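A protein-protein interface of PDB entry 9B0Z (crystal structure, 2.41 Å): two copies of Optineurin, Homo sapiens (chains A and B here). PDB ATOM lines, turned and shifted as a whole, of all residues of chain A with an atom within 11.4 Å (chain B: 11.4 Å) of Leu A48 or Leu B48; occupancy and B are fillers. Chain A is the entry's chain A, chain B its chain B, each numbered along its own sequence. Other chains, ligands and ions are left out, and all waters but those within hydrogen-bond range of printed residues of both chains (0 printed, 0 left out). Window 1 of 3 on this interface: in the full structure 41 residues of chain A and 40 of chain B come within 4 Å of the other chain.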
ATOM      1  N   GLU A  39       0.999  -9.646  10.032  1.00  0.00           N
ATOM      2  CA  GLU A  39       1.831 -10.370  10.990  1.00  0.00           C
ATOM      3  C   GLU A  39       0.994 -10.928  12.136  1.00  0.00           C
ATOM      4  O   GLU A  39       1.196 -12.074  12.560  1.00  0.00           O
ATOM      5  CB  GLU A  39       2.924  -9.452  11.537  1.00  0.00           C
ATOM      6  CG  GLU A  39       4.253  -9.495  10.801  1.00  0.00           C
ATOM      7  CD  GLU A  39       5.277  -8.582  11.458  1.00  0.00           C
ATOM      8  OE1 GLU A  39       6.272  -8.194  10.803  1.00  0.00           O
ATOM      9  OE2 GLU A  39       5.069  -8.243  12.642  1.00  0.00           O
ATOM     10  N   GLU A  40       0.044 -10.133  12.644  1.00  0.00           N
ATOM     11  CA  GLU A  40      -0.879 -10.631  13.661  1.00  0.00           C
ATOM     12  C   GLU A  40      -1.663 -11.834  13.153  1.00  0.00           C
ATOM     13  O   GLU A  40      -1.821 -12.829  13.871  1.00  0.00           O
ATOM     14  CB  GLU A  40      -1.838  -9.526  14.101  1.00  0.00           C
ATOM     15  CG  GLU A  40      -1.388  -8.740  15.321  1.00  0.00           C
ATOM     16  CD  GLU A  40      -2.451  -7.761  15.799  1.00  0.00           C
ATOM     17  OE1 GLU A  40      -2.626  -7.611  17.030  1.00  0.00           O
ATOM     18  OE2 GLU A  40      -3.122  -7.151  14.938  1.00  0.00           O
ATOM     19  N   ASP A  41      -2.151 -11.768  11.915  1.00  0.00           N
ATOM     20  CA  ASP A  41      -2.894 -12.894  11.360  1.00  0.00           C
ATOM     21  C   ASP A  41      -2.001 -14.123  11.226  1.00  0.00           C
ATOM     22  O   ASP A  41      -2.461 -15.254  11.425  1.00  0.00           O
ATOM     23  CB  ASP A  41      -3.493 -12.519  10.006  1.00  0.00           C
ATOM     24  CG  ASP A  41      -4.729 -11.646  10.133  1.00  0.00           C
ATOM     25  OD1 ASP A  41      -4.978 -11.100  11.231  1.00  0.00           O
ATOM     26  OD2 ASP A  41      -5.450 -11.502   9.121  1.00  0.00           O
ATOM     27  N   LEU A  42      -0.721 -13.924  10.875  1.00  0.00           N
ATOM     28  CA  LEU A  42       0.210 -15.044  10.829  1.00  0.00           C
ATOM     29  C   LEU A  42       0.530 -15.610  12.198  1.00  0.00           C
ATOM     30  O   LEU A  42       0.771 -16.819  12.301  1.00  0.00           O
ATOM     31  CB  LEU A  42       1.514 -14.659  10.123  1.00  0.00           C
ATOM     32  CG  LEU A  42       1.260 -14.734   8.616  1.00  0.00           C
ATOM     33  CD1 LEU A  42       2.623 -14.706   7.781  1.00  0.00           C
ATOM     34  CD2 LEU A  42       0.317 -15.916   8.274  1.00  0.00           C
ATOM     35  N   GLU A  43       0.442 -14.804  13.255  1.00  0.00           N
ATOM     36  CA  GLU A  43       0.526 -15.358  14.603  1.00  0.00           C
ATOM     37  C   GLU A  43      -0.581 -16.378  14.838  1.00  0.00           C
ATOM     38  O   GLU A  43      -0.339 -17.461  15.386  1.00  0.00           O
ATOM     39  CB  GLU A  43       0.479 -14.236  15.636  1.00  0.00           C
ATOM     40  CG  GLU A  43       0.719 -14.705  17.066  1.00  0.00           C
ATOM     41  CD  GLU A  43       1.734 -13.844  17.813  1.00  0.00           C
ATOM     42  OE1 GLU A  43       1.975 -14.108  19.014  1.00  0.00           O
ATOM     43  OE2 GLU A  43       2.291 -12.905  17.199  1.00  0.00           O
ATOM     44  N   THR A  44      -1.813 -16.045  14.437  1.00  0.00           N
ATOM     45  CA  THR A  44      -2.902 -16.999  14.599  1.00  0.00           C
ATOM     46  C   THR A  44      -2.621 -18.283  13.833  1.00  0.00           C
ATOM     47  O   THR A  44      -3.025 -19.361  14.281  1.00  0.00           O
ATOM     48  CB  THR A  44      -4.240 -16.386  14.179  1.00  0.00           C
ATOM     49  OG1 THR A  44      -4.064 -15.581  13.006  1.00  0.00           O
ATOM     50  CG2 THR A  44      -4.793 -15.525  15.311  1.00  0.00           C
ATOM     51  N   MET A  45      -1.912 -18.201  12.694  1.00  0.00           N
ATOM     52  CA  MET A  45      -1.657 -19.427  11.942  1.00  0.00           C
ATOM     53  C   MET A  45      -0.764 -20.371  12.724  1.00  0.00           C
ATOM     54  O   MET A  45      -0.994 -21.582  12.722  1.00  0.00           O
ATOM     55  CB  MET A  45      -1.012 -19.187  10.581  1.00  0.00           C
ATOM     56  CG  MET A  45      -1.988 -19.306   9.445  1.00  0.00           C
ATOM     57  SD  MET A  45      -1.228 -19.246   7.812  1.00  0.00           S
ATOM     58  CE  MET A  45       0.263 -20.211   8.117  1.00  0.00           C
ATOM     59  N   THR A  46       0.270 -19.839  13.376  1.00  0.00           N
ATOM     60  CA  THR A  46       1.138 -20.679  14.192  1.00  0.00           C
ATOM     61  C   THR A  46       0.351 -21.409  15.269  1.00  0.00           C
ATOM     62  O   THR A  46       0.631 -22.579  15.573  1.00  0.00           O
ATOM     63  CB  THR A  46       2.242 -19.825  14.810  1.00  0.00           C
ATOM     64  OG1 THR A  46       3.224 -19.521  13.812  1.00  0.00           O
ATOM     65  CG2 THR A  46       2.899 -20.536  15.994  1.00  0.00           C
ATOM     66  N   ILE A  47      -0.648 -20.744  15.845  1.00  0.00           N
ATOM     67  CA  ILE A  47      -1.454 -21.377  16.886  1.00  0.00           C
ATOM     68  C   ILE A  47      -2.407 -22.389  16.282  1.00  0.00           C
ATOM     69  O   ILE A  47      -2.635 -23.466  16.848  1.00  0.00           O
ATOM     70  CB  ILE A  47      -2.179 -20.300  17.713  1.00  0.00           C
ATOM     71  CG1 ILE A  47      -1.126 -19.343  18.259  1.00  0.00           C
ATOM     72  CG2 ILE A  47      -2.998 -20.926  18.817  1.00  0.00           C
ATOM     73  CD1 ILE A  47       0.093 -20.092  18.800  1.00  0.00           C
ATOM     74  N   LEU A  48      -2.953 -22.066  15.112  1.00  0.00           N
ATOM     75  CA  LEU A  48      -3.801 -23.000  14.390  1.00  0.00           C
ATOM     76  C   LEU A  48      -3.061 -24.310  14.144  1.00  0.00           C
ATOM     77  O   LEU A  48      -3.609 -25.396  14.373  1.00  0.00           O
ATOM     78  CB  LEU A  48      -4.231 -22.349  13.079  1.00  0.00           C
ATOM     79  CG  LEU A  48      -5.411 -22.867  12.280  1.00  0.00           C
ATOM     80  CD1 LEU A  48      -6.549 -23.242  13.192  1.00  0.00           C
ATOM     81  CD2 LEU A  48      -5.816 -21.744  11.368  1.00  0.00           C
ATOM     82  N   ARG A  49      -1.801 -24.226  13.709  1.00  0.00           N
ATOM     83  CA  ARG A  49      -0.981 -25.425  13.577  1.00  0.00           C
ATOM     84  C   ARG A  49      -0.830 -26.128  14.923  1.00  0.00           C
ATOM     85  O   ARG A  49      -1.057 -27.338  15.035  1.00  0.00           O
ATOM     86  CB  ARG A  49       0.393 -25.070  13.004  1.00  0.00           C
ATOM     87  CG  ARG A  49       0.447 -24.931  11.488  1.00  0.00           C
ATOM     88  CD  ARG A  49       1.860 -24.592  10.994  1.00  0.00           C
ATOM     89  N   ALA A  50      -0.461 -25.378  15.967  1.00  0.00           N
ATOM     90  CA  ALA A  50      -0.292 -25.980  17.288  1.00  0.00           C
ATOM     91  C   ALA A  50      -1.580 -26.625  17.774  1.00  0.00           C
ATOM     92  O   ALA A  50      -1.552 -27.680  18.422  1.00  0.00           O
ATOM     93  CB  ALA A  50       0.187 -24.938  18.292  1.00  0.00           C
ATOM     94  N   GLN A  51      -2.718 -25.998  17.481  1.00  0.00           N
ATOM     95  CA  GLN A  51      -4.003 -26.555  17.886  1.00  0.00           C
ATOM     96  C   GLN A  51      -4.251 -27.907  17.235  1.00  0.00           C
ATOM     97  O   GLN A  51      -4.478 -28.910  17.923  1.00  0.00           O
ATOM     98  CB  GLN A  51      -5.115 -25.590  17.491  1.00  0.00           C
ATOM     99  CG  GLN A  51      -6.501 -26.013  17.898  1.00  0.00           C
ATOM    100  CD  GLN A  51      -6.898 -25.487  19.244  1.00  0.00           C
ATOM    101  OE1 GLN A  51      -6.083 -25.426  20.163  1.00  0.00           O
ATOM    102  NE2 GLN A  51      -8.160 -25.085  19.372  1.00  0.00           N
ATOM    103  N   MET A  52      -4.172 -27.956  15.902  1.00  0.00           N
ATOM    104  CA  MET A  52      -4.492 -29.183  15.185  1.00  0.00           C
ATOM    105  C   MET A  52      -3.579 -30.329  15.592  1.00  0.00           C
ATOM    106  O   MET A  52      -4.021 -31.482  15.632  1.00  0.00           O
ATOM    107  CB  MET A  52      -4.435 -28.940  13.684  1.00  0.00           C
ATOM    108  CG  MET A  52      -3.043 -28.791  13.164  1.00  0.00           C
ATOM    109  SD  MET A  52      -3.076 -28.021  11.549  1.00  0.00           S
ATOM    110  CE  MET A  52      -3.443 -29.417  10.546  1.00  0.00           C
ATOM    111  N   GLU A  53      -2.320 -30.038  15.916  1.00  0.00           N
ATOM    112  CA  GLU A  53      -1.429 -31.098  16.374  1.00  0.00           C
ATOM    113  C   GLU A  53      -1.897 -31.662  17.710  1.00  0.00           C
ATOM    114  O   GLU A  53      -1.676 -32.846  17.995  1.00  0.00           O
ATOM    115  CB  GLU A  53       0.008 -30.582  16.468  1.00  0.00           C
ATOM    116  CG  GLU A  53       0.771 -30.679  15.152  1.00  0.00           C
ATOM    117  CD  GLU A  53       0.352 -31.885  14.318  1.00  0.00           C
ATOM    118  OE1 GLU A  53      -0.310 -31.688  13.273  1.00  0.00           O
ATOM    119  OE2 GLU A  53       0.677 -33.029  14.714  1.00  0.00           O
ATOM    120  N   VAL A  54      -2.531 -30.835  18.543  1.00  0.00           N
ATOM    121  CA  VAL A  54      -3.110 -31.346  19.783  1.00  0.00           C
ATOM    122  C   VAL A  54      -4.344 -32.192  19.490  1.00  0.00           C
ATOM    123  O   VAL A  54      -4.586 -33.215  20.148  1.00  0.00           O
ATOM    124  CB  VAL A  54      -3.429 -30.186  20.743  1.00  0.00           C
ATOM    125  CG1 VAL A  54      -4.566 -30.552  21.676  1.00  0.00           C
ATOM    126  CG2 VAL A  54      -2.203 -29.840  21.548  1.00  0.00           C
ATOM    127  N   TYR A  55      -5.133 -31.798  18.487  1.00  0.00           N
ATOM    128  CA  TYR A  55      -6.308 -32.586  18.129  1.00  0.00           C
ATOM    129  C   TYR A  55      -5.918 -33.992  17.689  1.00  0.00           C
ATOM    130  O   TYR A  55      -6.632 -34.960  17.980  1.00  0.00           O
ATOM    131  CB  TYR A  55      -7.117 -31.876  17.045  1.00  0.00           C
ATOM    132  CG  TYR A  55      -7.908 -30.681  17.546  1.00  0.00           C
ATOM    133  CD1 TYR A  55      -7.875 -30.309  18.885  1.00  0.00           C
ATOM    134  CD2 TYR A  55      -8.724 -29.954  16.688  1.00  0.00           C
ATOM    135  CE1 TYR A  55      -8.604 -29.221  19.348  1.00  0.00           C
ATOM    136  CE2 TYR A  55      -9.459 -28.872  17.140  1.00  0.00           C
ATOM    137  CZ  TYR A  55      -9.394 -28.507  18.471  1.00  0.00           C
ATOM    138  OH  TYR A  55     -10.120 -27.423  18.922  1.00  0.00           O
ATOM    139  N   CYS A  56      -4.782 -34.136  16.999  1.00  0.00           N
ATOM    140  CA  CYS A  56      -4.316 -35.477  16.660  1.00  0.00           C
ATOM    141  C   CYS A  56      -3.991 -36.262  17.916  1.00  0.00           C
ATOM    142  O   CYS A  56      -4.435 -37.404  18.081  1.00  0.00           O
ATOM    143  CB  CYS A  56      -3.086 -35.419  15.758  1.00  0.00           C
ATOM    144  SG  CYS A  56      -3.385 -34.675  14.182  1.00  0.00           S
ATOM    145  N   SER A  57      -3.248 -35.647  18.838  1.00  0.00           N
ATOM    146  CA  SER A  57      -2.922 -36.327  20.084  1.00  0.00           C
ATOM    147  C   SER A  57      -4.193 -36.807  20.763  1.00  0.00           C
ATOM    148  O   SER A  57      -4.234 -37.910  21.315  1.00  0.00           O
ATOM    149  CB  SER A  57      -2.162 -35.389  21.019  1.00  0.00           C
ATOM    150  OG  SER A  57      -1.156 -34.683  20.321  1.00  0.00           O
ATOM    151  N   GLU B  40       0.218 -14.586   0.311  1.00  0.00           N
ATOM    152  CA  GLU B  40       0.253 -15.961  -0.172  1.00  0.00           C
ATOM    153  C   GLU B  40       0.229 -16.945   0.990  1.00  0.00           C
ATOM    154  O   GLU B  40      -0.475 -17.959   0.937  1.00  0.00           O
ATOM    155  CB  GLU B  40       1.492 -16.194  -1.034  1.00  0.00           C
ATOM    156  N   ASP B  41       0.999 -16.670   2.046  1.00  0.00           N
ATOM    157  CA  ASP B  41       1.006 -17.566   3.199  1.00  0.00           C
ATOM    158  C   ASP B  41      -0.341 -17.581   3.908  1.00  0.00           C
ATOM    159  O   ASP B  41      -0.754 -18.637   4.404  1.00  0.00           O
ATOM    160  CB  ASP B  41       2.131 -17.199   4.153  1.00  0.00           C
ATOM    161  CG  ASP B  41       3.478 -17.684   3.657  1.00  0.00           C
ATOM    162  OD1 ASP B  41       3.577 -18.050   2.462  1.00  0.00           O
ATOM    163  OD2 ASP B  41       4.429 -17.729   4.463  1.00  0.00           O
ATOM    164  N   LEU B  42      -1.052 -16.441   3.935  1.00  0.00           N
ATOM    165  CA  LEU B  42      -2.394 -16.401   4.510  1.00  0.00           C
ATOM    166  C   LEU B  42      -3.378 -17.278   3.755  1.00  0.00           C
ATOM    167  O   LEU B  42      -4.389 -17.685   4.337  1.00  0.00           O
ATOM    168  CB  LEU B  42      -2.981 -14.985   4.528  1.00  0.00           C
ATOM    169  CG  LEU B  42      -2.594 -13.967   5.611  1.00  0.00           C
ATOM    170  CD1 LEU B  42      -3.090 -14.449   6.912  1.00  0.00           C
ATOM    171  CD2 LEU B  42      -1.165 -13.586   5.760  1.00  0.00           C
ATOM    172  N   GLU B  43      -3.102 -17.592   2.488  1.00  0.00           N
ATOM    173  CA  GLU B  43      -3.915 -18.572   1.773  1.00  0.00           C
ATOM    174  C   GLU B  43      -3.936 -19.894   2.521  1.00  0.00           C
ATOM    175  O   GLU B  43      -4.982 -20.546   2.624  1.00  0.00           O
ATOM    176  CB  GLU B  43      -3.396 -18.764   0.349  1.00  0.00           C
ATOM    177  CG  GLU B  43      -3.420 -17.519  -0.536  1.00  0.00           C
ATOM    178  CD  GLU B  43      -2.714 -17.753  -1.869  1.00  0.00           C
ATOM    179  OE1 GLU B  43      -2.438 -18.929  -2.193  1.00  0.00           O
ATOM    180  OE2 GLU B  43      -2.425 -16.769  -2.587  1.00  0.00           O
ATOM    181  N   THR B  44      -2.782 -20.296   3.055  1.00  0.00           N
ATOM    182  CA  THR B  44      -2.667 -21.551   3.789  1.00  0.00           C
ATOM    183  C   THR B  44      -3.624 -21.625   4.974  1.00  0.00           C
ATOM    184  O   THR B  44      -4.115 -22.712   5.299  1.00  0.00           O
ATOM    185  CB  THR B  44      -1.216 -21.732   4.256  1.00  0.00           C
ATOM    186  OG1 THR B  44      -0.402 -22.176   3.163  1.00  0.00           O
ATOM    187  CG2 THR B  44      -1.108 -22.728   5.401  1.00  0.00           C
ATOM    188  N   MET B  45      -3.948 -20.487   5.596  1.00  0.00           N
ATOM    189  CA  MET B  45      -4.722 -20.528   6.836  1.00  0.00           C
ATOM    190  C   MET B  45      -6.107 -21.127   6.619  1.00  0.00           C
ATOM    191  O   MET B  45      -6.585 -21.909   7.450  1.00  0.00           O
ATOM    192  CB  MET B  45      -4.804 -19.137   7.465  1.00  0.00           C
ATOM    193  CG  MET B  45      -5.349 -19.167   8.887  1.00  0.00           C
ATOM    194  SD  MET B  45      -5.036 -17.671   9.850  1.00  0.00           S
ATOM    195  CE  MET B  45      -5.315 -16.416   8.629  1.00  0.00           C
ATOM    196  N   THR B  46      -6.766 -20.790   5.507  1.00  0.00           N
ATOM    197  CA  THR B  46      -8.049 -21.428   5.202  1.00  0.00           C
ATOM    198  C   THR B  46      -7.910 -22.949   5.109  1.00  0.00           C
ATOM    199  O   THR B  46      -8.855 -23.680   5.435  1.00  0.00           O
ATOM    200  CB  THR B  46      -8.671 -20.852   3.925  1.00  0.00           C
ATOM    201  OG1 THR B  46     -10.073 -21.153   3.903  1.00  0.00           O
ATOM    202  CG2 THR B  46      -8.045 -21.431   2.667  1.00  0.00           C
ATOM    203  N   ILE B  47      -6.757 -23.447   4.644  1.00  0.00           N
ATOM    204  CA  ILE B  47      -6.555 -24.890   4.562  1.00  0.00           C
ATOM    205  C   ILE B  47      -6.312 -25.476   5.950  1.00  0.00           C
ATOM    206  O   ILE B  47      -6.801 -26.568   6.277  1.00  0.00           O
ATOM    207  CB  ILE B  47      -5.388 -25.216   3.619  1.00  0.00           C
ATOM    208  CG1 ILE B  47      -5.578 -24.535   2.257  1.00  0.00           C
ATOM    209  CG2 ILE B  47      -5.281 -26.730   3.437  1.00  0.00           C
ATOM    210  CD1 ILE B  47      -6.965 -24.694   1.673  1.00  0.00           C
ATOM    211  N   LEU B  48      -5.542 -24.774   6.789  1.00  0.00           N
ATOM    212  CA  LEU B  48      -5.317 -25.234   8.160  1.00  0.00           C
ATOM    213  C   LEU B  48      -6.624 -25.339   8.929  1.00  0.00           C
ATOM    214  O   LEU B  48      -6.875 -26.339   9.609  1.00  0.00           O
ATOM    215  CB  LEU B  48      -4.369 -24.284   8.881  1.00  0.00           C
ATOM    216  CG  LEU B  48      -2.937 -24.735   9.116  1.00  0.00           C
ATOM    217  CD1 LEU B  48      -2.369 -25.277   7.844  1.00  0.00           C
ATOM    218  CD2 LEU B  48      -2.161 -23.522   9.549  1.00  0.00           C
ATOM    219  N   ARG B  49      -7.474 -24.313   8.835  1.00  0.00           N
ATOM    220  CA  ARG B  49      -8.749 -24.362   9.542  1.00  0.00           C
ATOM    221  C   ARG B  49      -9.555 -25.576   9.112  1.00  0.00           C
ATOM    222  O   ARG B  49     -10.040 -26.342   9.952  1.00  0.00           O
ATOM    223  CB  ARG B  49      -9.551 -23.077   9.310  1.00  0.00           C
ATOM    224  CG  ARG B  49      -8.948 -21.834   9.941  1.00  0.00           C
ATOM    225  CD  ARG B  49      -9.999 -20.832  10.411  1.00  0.00           C
ATOM    226  NE  ARG B  49      -9.408 -19.620  10.975  1.00  0.00           N
ATOM    227  CZ  ARG B  49      -9.372 -19.327  12.270  1.00  0.00           C
ATOM    228  NH1 ARG B  49      -9.867 -20.151  13.182  1.00  0.00           N
ATOM    229  NH2 ARG B  49      -8.835 -18.171  12.658  1.00  0.00           N
ATOM    230  N   ALA B  50      -9.682 -25.785   7.800  1.00  0.00           N
ATOM    231  CA  ALA B  50     -10.437 -26.933   7.306  1.00  0.00           C
ATOM    232  C   ALA B  50      -9.849 -28.233   7.822  1.00  0.00           C
ATOM    233  O   ALA B  50     -10.587 -29.161   8.174  1.00  0.00           O
ATOM    234  CB  ALA B  50     -10.460 -26.939   5.780  1.00  0.00           C
ATOM    235  N   GLN B  51      -8.520 -28.320   7.874  1.00  0.00           N
ATOM    236  CA  GLN B  51      -7.884 -29.519   8.401  1.00  0.00           C
ATOM    237  C   GLN B  51      -8.225 -29.703   9.875  1.00  0.00           C
ATOM    238  O   GLN B  51      -8.514 -30.818  10.325  1.00  0.00           O
ATOM    239  CB  GLN B  51      -6.376 -29.468   8.204  1.00  0.00           C
ATOM    240  CG  GLN B  51      -5.732 -30.805   8.576  1.00  0.00           C
ATOM    241  CD  GLN B  51      -5.593 -31.765   7.402  1.00  0.00           C
ATOM    242  OE1 GLN B  51      -6.363 -32.724   7.253  1.00  0.00           O
ATOM    243  NE2 GLN B  51      -4.594 -31.511   6.562  1.00  0.00           N
ATOM    244  N   MET B  52      -8.124 -28.628  10.660  1.00  0.00           N
ATOM    245  CA  MET B  52      -8.447 -28.730  12.077  1.00  0.00           C
ATOM    246  C   MET B  52      -9.881 -29.216  12.264  1.00  0.00           C
ATOM    247  O   MET B  52     -10.157 -30.024  13.156  1.00  0.00           O
ATOM    248  CB  MET B  52      -8.222 -27.371  12.751  1.00  0.00           C
ATOM    249  CG  MET B  52      -8.054 -27.371  14.277  1.00  0.00           C
ATOM    250  SD  MET B  52      -8.273 -25.716  15.026  1.00  0.00           S
ATOM    251  CE  MET B  52     -10.053 -25.439  14.968  1.00  0.00           C
ATOM    252  N   GLU B  53     -10.796 -28.799  11.383  1.00  0.00           N
ATOM    253  CA  GLU B  53     -12.171 -29.280  11.490  1.00  0.00           C
ATOM    254  C   GLU B  53     -12.299 -30.772  11.179  1.00  0.00           C
ATOM    255  O   GLU B  53     -13.152 -31.446  11.770  1.00  0.00           O
ATOM    256  CB  GLU B  53     -13.104 -28.463  10.592  1.00  0.00           C
ATOM    257  CG  GLU B  53     -13.652 -27.222  11.281  1.00  0.00           C
ATOM    258  CD  GLU B  53     -13.513 -25.960  10.445  1.00  0.00           C
ATOM    259  OE1 GLU B  53     -13.820 -25.999   9.231  1.00  0.00           O
ATOM    260  OE2 GLU B  53     -13.095 -24.924  11.011  1.00  0.00           O
ATOM    261  N   VAL B  54     -11.492 -31.317  10.264  1.00  0.00           N
ATOM    262  CA  VAL B  54     -11.577 -32.762  10.045  1.00  0.00           C
ATOM    263  C   VAL B  54     -10.969 -33.517  11.224  1.00  0.00           C
ATOM    264  O   VAL B  54     -11.485 -34.564  11.634  1.00  0.00           O
ATOM    265  CB  VAL B  54     -10.956 -33.188   8.694  1.00  0.00           C
ATOM    266  CG1 VAL B  54     -11.377 -32.241   7.574  1.00  0.00           C
ATOM    267  CG2 VAL B  54      -9.447 -33.298   8.764  1.00  0.00           C
ATOM    268  N   TYR B  55      -9.884 -32.994  11.806  1.00  0.00           N
ATOM    269  CA  TYR B  55      -9.304 -33.637  12.984  1.00  0.00           C
ATOM    270  C   TYR B  55     -10.297 -33.619  14.131  1.00  0.00           C
ATOM    271  O   TYR B  55     -10.405 -34.588  14.893  1.00  0.00           O
ATOM    272  CB  TYR B  55      -8.002 -32.940  13.378  1.00  0.00           C
ATOM    273  CG  TYR B  55      -6.840 -33.261  12.450  1.00  0.00           C
ATOM    274  CD1 TYR B  55      -6.985 -34.183  11.418  1.00  0.00           C
ATOM    275  CD2 TYR B  55      -5.617 -32.625  12.585  1.00  0.00           C
ATOM    276  CE1 TYR B  55      -5.942 -34.473  10.566  1.00  0.00           C
ATOM    277  CE2 TYR B  55      -4.566 -32.903  11.723  1.00  0.00           C
ATOM    278  CZ  TYR B  55      -4.736 -33.834  10.720  1.00  0.00           C
ATOM    279  OH  TYR B  55      -3.702 -34.136   9.856  1.00  0.00           O
ATOM    280  N   CYS B  56     -11.059 -32.536  14.242  1.00  0.00           N
ATOM    281  CA  CYS B  56     -12.091 -32.451  15.264  1.00  0.00           C
ATOM    282  C   CYS B  56     -13.191 -33.487  15.033  1.00  0.00           C
ATOM    283  O   CYS B  56     -13.555 -34.227  15.951  1.00  0.00           O
ATOM    284  CB  CYS B  56     -12.664 -31.032  15.278  1.00  0.00           C
ATOM    285  SG  CYS B  56     -13.723 -30.719  16.683  1.00  0.00           S
ATOM    286  N   SER B  57     -13.727 -33.566  13.810  1.00  0.00           N
ATOM    287  CA  SER B  57     -14.751 -34.570  13.518  1.00  0.00           C
ATOM    288  C   SER B  57     -14.230 -35.974  13.772  1.00  0.00           C
ATOM    289  O   SER B  57     -14.962 -36.842  14.269  1.00  0.00           O
ATOM    290  CB  SER B  57     -15.240 -34.438  12.075  1.00  0.00           C
ATOM    291  OG  SER B  57     -15.545 -33.093  11.757  1.00  0.00           O
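Asp A41 touches Leu B42, but with the chains exchanged Leu A42 does not touch Asp B41 (4.4 Å).
Leu A48 touches Met B52, but with the chains exchanged Met A52 does not touch Leu B48 (4.1 Å).
Met A52 touches its own counterpart, Met B52.
Met A52 touches Tyr B55, and with the chains exchanged Tyr A55 touches Met B52.
Positions printed for both chains: 40, 41, 42, 43, 44, 45, 46, 47, 48, 49, 50, 51, 52, 53, 54, 55, 56 and 57.
Of the 20 pairs that touch across the chains among the printed residues, 17 have their exchanged pair printed and touching as well.
Of the 19 printed residues of chain A, 10 touch a printed residue of chain B.
Hydrophobic or aromatic side chains of chain A within 4 Å of the printed part of chain B: Leu A42, Met A45, Leu A48, Met A52 and Tyr A55.
Hydrophobic or aromatic side chains of chain B that line the printed part of chain A: Leu B42, Met B45, Leu B48, Met B52 and Tyr B55.
Along chain B the printed residues that touch a printed residue of chain A span positions 41 to 55.
Among the printed residues, 20 pairs touch across the chains.
Among the printed residues, no Asp or Glu carboxylate lies within 4 Å of a Lys or Arg side-chain nitrogen of the other chain.
The backbone carbonyl oxygen (O) of Asp B41 sits close to the side-chain sulfur (SD) of Met A45 (3.5 Å).
N of Met B45 sits close to SD of Met A45.
The side-chain sulfur of Cys A56 lies within hydrogen-bond range of the backbone carbonyl oxygen of Met A52 (3.6 Å).
The side-chain amide nitrogen (NE2) of Gln A51 lies within hydrogen-bond range of the side-chain hydroxyl (OH) of Tyr A55.
Of chain B, only Met B45, Leu B48, Arg B49 and Met B52 come within 4 Å of Leu A48.
Leu B48 touches just these residues of chain A: Met A45 (3.9 Å), Leu A48 (3.8 Å) and Arg A49 (3.5 Å).
Of the printed residues of chain B, Met A45 touches Asp B41 (3.5 Å), Thr B44 (3.9 Å), Met B45 (3.4 Å) and Leu B48 (3.9 Å).
No residue of chain B comes within 4 Å of Thr A46.
No residue of chain B comes within 4 Å of Ala A50.
Thr B44 touches one residue of chain A.
Met B45 touches four residues of chain A.
Arg B49 touches just one residue of chain A: Leu A48 (3.4 Å).
No residue of chain A comes within 4 Å of Ala B50.
Printed residues of chain B within 4 Å of Asp A41: Leu B42 and Met B45.
Of the printed residues of chain A, Tyr B55 touches Met A52, Tyr A55 and Cys A56.
Printed residues of chain A within 4 Å of Asp B41: Met A45.
Glu A40 touches none of the printed residues of chain B.
The nearest residue of chain A that does not touch Leu B48 is Met A52 (4.1 Å).
The nearest printed residue of chain A that does not touch Tyr B55 is Glu A53 (4.7 Å).
Met B45 touches Asp A41 (SD to O, 3.9 Å).
Leu A42 touches Leu B42.
Met B45 touches Thr A44 (SD to OG1, 3.9 Å).
Met A45 touches Thr B44.
Leu A48 touches Met B45.
Leu A48 touches Leu B48.
CG of Arg A49 touches CD2 of Leu B48, 3.5 Å away.
Met B52 touches Met A52 (CG to CB, 3.99 Å).
CG of Met B52 touches CE2 of Tyr A55 (3.5 Å).
Tyr B55 touches Tyr A55.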
